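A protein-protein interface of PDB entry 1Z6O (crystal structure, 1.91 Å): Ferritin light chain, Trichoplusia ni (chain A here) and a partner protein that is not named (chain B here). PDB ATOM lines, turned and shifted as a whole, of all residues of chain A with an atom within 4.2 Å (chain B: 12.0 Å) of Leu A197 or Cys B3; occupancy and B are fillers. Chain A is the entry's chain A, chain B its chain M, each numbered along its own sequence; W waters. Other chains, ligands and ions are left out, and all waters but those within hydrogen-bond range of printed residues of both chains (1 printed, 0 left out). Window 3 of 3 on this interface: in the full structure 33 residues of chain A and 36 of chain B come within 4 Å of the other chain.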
ATOM      1  N   HIS A 121     -20.991  -6.176  -8.156  1.00  0.00           N
ATOM      2  CA  HIS A 121     -20.708  -6.595  -6.795  1.00  0.00           C
ATOM      3  C   HIS A 121     -21.889  -7.528  -6.448  1.00  0.00           C
ATOM      4  O   HIS A 121     -22.859  -7.613  -7.209  1.00  0.00           O
ATOM      5  CB  HIS A 121     -20.583  -5.393  -5.835  1.00  0.00           C
ATOM      6  CG  HIS A 121     -21.798  -4.519  -5.743  1.00  0.00           C
ATOM      7  ND1 HIS A 121     -21.757  -3.170  -6.035  1.00  0.00           N
ATOM      8  CD2 HIS A 121     -23.047  -4.763  -5.278  1.00  0.00           C
ATOM      9  CE1 HIS A 121     -22.924  -2.623  -5.747  1.00  0.00           C
ATOM     10  NE2 HIS A 121     -23.725  -3.568  -5.286  1.00  0.00           N
ATOM     11  N   PHE A 188     -26.892  -6.953   5.853  1.00  0.00           N
ATOM     12  CA  PHE A 188     -25.450  -7.025   6.128  1.00  0.00           C
ATOM     13  C   PHE A 188     -24.825  -5.657   5.874  1.00  0.00           C
ATOM     14  O   PHE A 188     -23.889  -5.240   6.556  1.00  0.00           O
ATOM     15  CB  PHE A 188     -24.749  -8.018   5.191  1.00  0.00           C
ATOM     16  CG  PHE A 188     -25.182  -9.453   5.362  1.00  0.00           C
ATOM     17  CD1 PHE A 188     -25.145 -10.323   4.277  1.00  0.00           C
ATOM     18  CD2 PHE A 188     -25.584  -9.943   6.606  1.00  0.00           C
ATOM     19  CE1 PHE A 188     -25.501 -11.670   4.417  1.00  0.00           C
ATOM     20  CE2 PHE A 188     -25.942 -11.293   6.761  1.00  0.00           C
ATOM     21  CZ  PHE A 188     -25.899 -12.154   5.662  1.00  0.00           C
ATOM     22  N   ILE A 189     -25.339  -4.969   4.862  1.00  0.00           N
ATOM     23  CA  ILE A 189     -24.811  -3.664   4.490  1.00  0.00           C
ATOM     24  C   ILE A 189     -25.224  -2.554   5.450  1.00  0.00           C
ATOM     25  O   ILE A 189     -24.428  -1.670   5.756  1.00  0.00           O
ATOM     26  CB  ILE A 189     -25.278  -3.286   3.049  1.00  0.00           C
ATOM     27  CG1 ILE A 189     -24.570  -4.186   2.033  1.00  0.00           C
ATOM     28  CG2 ILE A 189     -25.018  -1.788   2.758  1.00  0.00           C
ATOM     29  CD1 ILE A 189     -25.220  -4.175   0.645  1.00  0.00           C
ATOM     30  N   GLY A 194     -22.729  -1.492   8.714  1.00  0.00           N
ATOM     31  CA  GLY A 194     -22.110  -2.341   7.707  1.00  0.00           C
ATOM     32  C   GLY A 194     -20.762  -2.915   8.104  1.00  0.00           C
ATOM     33  O   GLY A 194     -20.019  -3.411   7.253  1.00  0.00           O
ATOM     34  N   HIS A 195     -20.446  -2.882   9.395  1.00  0.00           N
ATOM     35  CA  HIS A 195     -19.160  -3.390   9.873  1.00  0.00           C
ATOM     36  C   HIS A 195     -18.857  -4.862   9.617  1.00  0.00           C
ATOM     37  O   HIS A 195     -17.697  -5.242   9.499  1.00  0.00           O
ATOM     38  CB  HIS A 195     -19.005  -3.123  11.376  1.00  0.00           C
ATOM     39  CG  HIS A 195     -18.675  -1.702  11.705  1.00  0.00           C
ATOM     40  ND1 HIS A 195     -17.835  -0.936  10.926  1.00  0.00           N
ATOM     41  CD2 HIS A 195     -19.072  -0.905  12.726  1.00  0.00           C
ATOM     42  CE1 HIS A 195     -17.732   0.273  11.449  1.00  0.00           C
ATOM     43  NE2 HIS A 195     -18.472   0.318  12.542  1.00  0.00           N
ATOM     44  N   ASP A 196     -19.882  -5.700   9.554  1.00  0.00           N
ATOM     45  CA  ASP A 196     -19.645  -7.118   9.324  1.00  0.00           C
ATOM     46  C   ASP A 196     -19.710  -7.510   7.852  1.00  0.00           C
ATOM     47  O   ASP A 196     -19.623  -8.693   7.526  1.00  0.00           O
ATOM     48  CB  ASP A 196     -20.674  -7.949  10.093  1.00  0.00           C
ATOM     49  CG  ASP A 196     -20.365  -8.027  11.583  1.00  0.00           C
ATOM     50  OD1 ASP A 196     -19.329  -7.475  12.006  1.00  0.00           O
ATOM     51  OD2 ASP A 196     -21.153  -8.644  12.325  1.00  0.00           O
ATOM     52  N   LEU A 197     -19.838  -6.533   6.962  1.00  0.00           N
ATOM     53  CA  LEU A 197     -20.002  -6.863   5.547  1.00  0.00           C
ATOM     54  C   LEU A 197     -19.054  -7.884   4.918  1.00  0.00           C
ATOM     55  O   LEU A 197     -19.514  -8.832   4.288  1.00  0.00           O
ATOM     56  CB  LEU A 197     -20.004  -5.589   4.686  1.00  0.00           C
ATOM     57  CG  LEU A 197     -20.349  -5.834   3.204  1.00  0.00           C
ATOM     58  CD1 LEU A 197     -21.739  -6.489   3.076  1.00  0.00           C
ATOM     59  CD2 LEU A 197     -20.321  -4.500   2.442  1.00  0.00           C
ATOM     60  N   SER A 198     -17.740  -7.721   5.073  1.00  0.00           N
ATOM     61  CA  SER A 198     -16.850  -8.675   4.417  1.00  0.00           C
ATOM     62  C   SER A 198     -17.002 -10.091   4.968  1.00  0.00           C
ATOM     63  O   SER A 198     -17.008 -11.063   4.207  1.00  0.00           O
ATOM     64  CB  SER A 198     -15.385  -8.206   4.495  1.00  0.00           C
ATOM     65  OG  SER A 198     -14.888  -8.323   5.815  1.00  0.00           O
ATOM     66  N   LEU A 199     -17.136 -10.227   6.282  1.00  0.00           N
ATOM     67  CA  LEU A 199     -17.304 -11.565   6.848  1.00  0.00           C
ATOM     68  C   LEU A 199     -18.670 -12.124   6.445  1.00  0.00           C
ATOM     69  O   LEU A 199     -18.812 -13.320   6.182  1.00  0.00           O
ATOM     70  CB  LEU A 199     -17.203 -11.522   8.378  1.00  0.00           C
ATOM     71  CG  LEU A 199     -17.312 -12.873   9.097  1.00  0.00           C
ATOM     72  CD1 LEU A 199     -16.164 -13.792   8.670  1.00  0.00           C
ATOM     73  CD2 LEU A 199     -17.274 -12.640  10.620  1.00  0.00           C
ATOM     74  N   ALA A 200     -19.680 -11.260   6.399  1.00  0.00           N
ATOM     75  CA  ALA A 200     -21.022 -11.712   6.026  1.00  0.00           C
ATOM     76  C   ALA A 200     -21.080 -12.203   4.578  1.00  0.00           C
ATOM     77  O   ALA A 200     -21.748 -13.204   4.292  1.00  0.00           O
ATOM     78  CB  ALA A 200     -22.054 -10.584   6.250  1.00  0.00           C
ATOM     79  N   LEU A 201     -20.393 -11.518   3.662  1.00  0.00           N
ATOM     80  CA  LEU A 201     -20.403 -11.961   2.260  1.00  0.00           C
ATOM     81  C   LEU A 201     -19.746 -13.332   2.142  1.00  0.00           C
ATOM     82  O   LEU A 201     -20.188 -14.182   1.367  1.00  0.00           O
ATOM     83  CB  LEU A 201     -19.682 -10.956   1.351  1.00  0.00           C
ATOM     84  CG  LEU A 201     -20.464  -9.642   1.165  1.00  0.00           C
ATOM     85  CD1 LEU A 201     -19.649  -8.641   0.353  1.00  0.00           C
ATOM     86  CD2 LEU A 201     -21.783  -9.929   0.468  1.00  0.00           C
ATOM     87  N   THR B   1     -24.165   4.993   0.173  1.00  0.00           N
ATOM     88  CA  THR B   1     -23.942   3.797   1.039  1.00  0.00           C
ATOM     89  C   THR B   1     -22.877   2.868   0.458  1.00  0.00           C
ATOM     90  O   THR B   1     -22.738   2.757  -0.764  1.00  0.00           O
ATOM     91  CB  THR B   1     -25.249   2.999   1.218  1.00  0.00           C
ATOM     92  OG1 THR B   1     -26.280   3.871   1.699  1.00  0.00           O
ATOM     93  CG2 THR B   1     -25.056   1.872   2.214  1.00  0.00           C
ATOM     94  N   GLN B   2     -22.128   2.208   1.339  1.00  0.00           N
ATOM     95  CA  GLN B   2     -21.069   1.286   0.930  1.00  0.00           C
ATOM     96  C   GLN B   2     -21.633  -0.129   0.774  1.00  0.00           C
ATOM     97  O   GLN B   2     -21.707  -0.883   1.746  1.00  0.00           O
ATOM     98  CB  GLN B   2     -19.955   1.285   1.983  1.00  0.00           C
ATOM     99  CG  GLN B   2     -18.789   0.355   1.672  1.00  0.00           C
ATOM    100  CD  GLN B   2     -18.103   0.711   0.372  1.00  0.00           C
ATOM    101  OE1 GLN B   2     -18.733   0.742  -0.688  1.00  0.00           O
ATOM    102  NE2 GLN B   2     -16.802   0.983   0.443  1.00  0.00           N
ATOM    103  N   CYS B   3     -22.011  -0.496  -0.445  1.00  0.00           N
ATOM    104  CA  CYS B   3     -22.590  -1.816  -0.676  1.00  0.00           C
ATOM    105  C   CYS B   3     -21.601  -2.900  -1.010  1.00  0.00           C
ATOM    106  O   CYS B   3     -21.965  -4.071  -1.075  1.00  0.00           O
ATOM    107  CB  CYS B   3     -23.636  -1.745  -1.781  1.00  0.00           C
ATOM    108  SG  CYS B   3     -24.986  -0.601  -1.355  1.00  0.00           S
ATOM    109  N   ASN B   4     -20.350  -2.526  -1.233  1.00  0.00           N
ATOM    110  CA  ASN B   4     -19.359  -3.531  -1.557  1.00  0.00           C
ATOM    111  C   ASN B   4     -18.104  -3.362  -0.720  1.00  0.00           C
ATOM    112  O   ASN B   4     -17.884  -2.332  -0.088  1.00  0.00           O
ATOM    113  CB  ASN B   4     -19.002  -3.478  -3.042  1.00  0.00           C
ATOM    114  CG  ASN B   4     -18.432  -2.143  -3.450  1.00  0.00           C
ATOM    115  OD1 ASN B   4     -19.156  -1.154  -3.571  1.00  0.00           O
ATOM    116  ND2 ASN B   4     -17.123  -2.102  -3.651  1.00  0.00           N
ATOM    117  N   VAL B   5     -17.281  -4.395  -0.725  1.00  0.00           N
ATOM    118  CA  VAL B   5     -16.050  -4.377   0.037  1.00  0.00           C
ATOM    119  C   VAL B   5     -14.898  -3.794  -0.772  1.00  0.00           C
ATOM    120  O   VAL B   5     -14.742  -4.110  -1.954  1.00  0.00           O
ATOM    121  CB  VAL B   5     -15.702  -5.794   0.464  1.00  0.00           C
ATOM    122  CG1 VAL B   5     -16.806  -6.330   1.373  1.00  0.00           C
ATOM    123  CG2 VAL B   5     -15.557  -6.686  -0.777  1.00  0.00           C
ATOM    124  N   ASN B   6     -14.110  -2.927  -0.138  1.00  0.00           N
ATOM    125  CA  ASN B   6     -12.957  -2.320  -0.800  1.00  0.00           C
ATOM    126  C   ASN B   6     -12.092  -3.477  -1.271  1.00  0.00           C
ATOM    127  O   ASN B   6     -11.701  -4.331  -0.476  1.00  0.00           O
ATOM    128  CB  ASN B   6     -12.168  -1.448   0.178  1.00  0.00           C
ATOM    129  CG  ASN B   6     -12.952  -0.234   0.635  1.00  0.00           C
ATOM    130  OD1 ASN B   6     -13.218   0.678  -0.150  1.00  0.00           O
ATOM    131  ND2 ASN B   6     -13.332  -0.219   1.912  1.00  0.00           N
ATOM    132  N   PRO B   7     -11.792  -3.527  -2.574  1.00  0.00           N
ATOM    133  CA  PRO B   7     -10.972  -4.607  -3.127  1.00  0.00           C
ATOM    134  C   PRO B   7      -9.579  -4.729  -2.503  1.00  0.00           C
ATOM    135  O   PRO B   7      -9.024  -3.763  -1.972  1.00  0.00           O
ATOM    136  CB  PRO B   7     -10.926  -4.273  -4.616  1.00  0.00           C
ATOM    137  CG  PRO B   7     -10.982  -2.771  -4.615  1.00  0.00           C
ATOM    138  CD  PRO B   7     -12.053  -2.490  -3.589  1.00  0.00           C
ATOM    139  N   VAL B   8      -9.037  -5.940  -2.551  1.00  0.00           N
ATOM    140  CA  VAL B   8      -7.710  -6.209  -2.020  1.00  0.00           C
ATOM    141  C   VAL B   8      -6.866  -6.649  -3.199  1.00  0.00           C
ATOM    142  O   VAL B   8      -7.387  -7.028  -4.245  1.00  0.00           O
ATOM    143  CB  VAL B   8      -7.722  -7.341  -0.965  1.00  0.00           C
ATOM    144  CG1 VAL B   8      -8.506  -6.895   0.268  1.00  0.00           C
ATOM    145  CG2 VAL B   8      -8.320  -8.619  -1.575  1.00  0.00           C
HETATM  146  O   HOH W   1     -21.968  -0.733   4.442  1.00  0.00           O
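O of Ile A189 lies close to N of Gly A194 (3.4 Å).
The side-chain amide oxygen of Gln B2 sits close to the backbone carbonyl oxygen of Asn B4, 3.2 Å away.
NE2 of His A121 touches CB of Cys B3, 3.95 Å away.
Asn B4 touches His A121 (CB to CB, 3.7 Å).
CG2 of Ile A189 touches CG2 of Thr B1 (3.7 Å).
Gln B2 touches Ile A189 (O to CG2, 3.6 Å).
CD1 of Ile A189 touches O of Cys B3, 3.7 Å away.
O of Gln B2 touches CD2 of Leu A197 (3.9 Å).
Leu A197 touches Cys B3.
Ser A198 touches Val B5.
Val B5 touches Leu A201.
Water W1 bridges O of Gln B2 (2.7 Å) and O of Ile A189 (2.9 Å).
His A121 touches just these residues of chain B: Cys B3 and Asn B4.
No residue of chain B comes within 4 Å of Phe A188.
Of the printed residues of chain B, Ile A189 touches Thr B1 (3.7 Å), Gln B2 (3.6 Å) and Cys B3 (3.7 Å).
No residue of chain B comes within 4 Å of Gly A194.
No residue of chain B comes within 4 Å of Asp A196.
No residue of chain B comes within 4 Å of Leu A199.
Of chain B, only Val B5 (3.8 Å) comes within 4 Å of Leu A201.
Of the printed residues of chain A, Thr B1 touches Ile A189 (3.7 Å).
Of the printed residues of chain A, Gln B2 touches Ile A189 and Leu A197.
Cys B3 touches just these residues of chain A: His A121 (3.95 Å), Ile A189 (3.7 Å) and Leu A197 (3.9 Å).
Of the printed residues of chain A, Asn B4 touches His A121 (3.7 Å).
Of the printed residues of chain A, Val B5 touches Ser A198 (3.8 Å) and Leu A201 (3.8 Å).
Val B8 touches none of the printed residues of chain A.
The nearest printed residue of chain A that does not touch Asn B4 is Leu A197 (4.03 Å).
Of the 11 printed residues of chain A, 5 touch a printed residue of chain B.
Printed residues of chain A that touch a printed residue of chain B: His A121, Ile A189, Leu A197, Ser A198 and Leu A201.
Hydrophobic or aromatic side chains of chain A that line the printed part of chain B: His A121, Ile A189, Leu A197 and Leu A201.
Of the 8 printed residues of chain B, 5 touch a printed residue of chain A.
Among the printed residues, no Asp or Glu carboxylate lies within 4 Å of a Lys or Arg side-chain nitrogen of the other chain.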
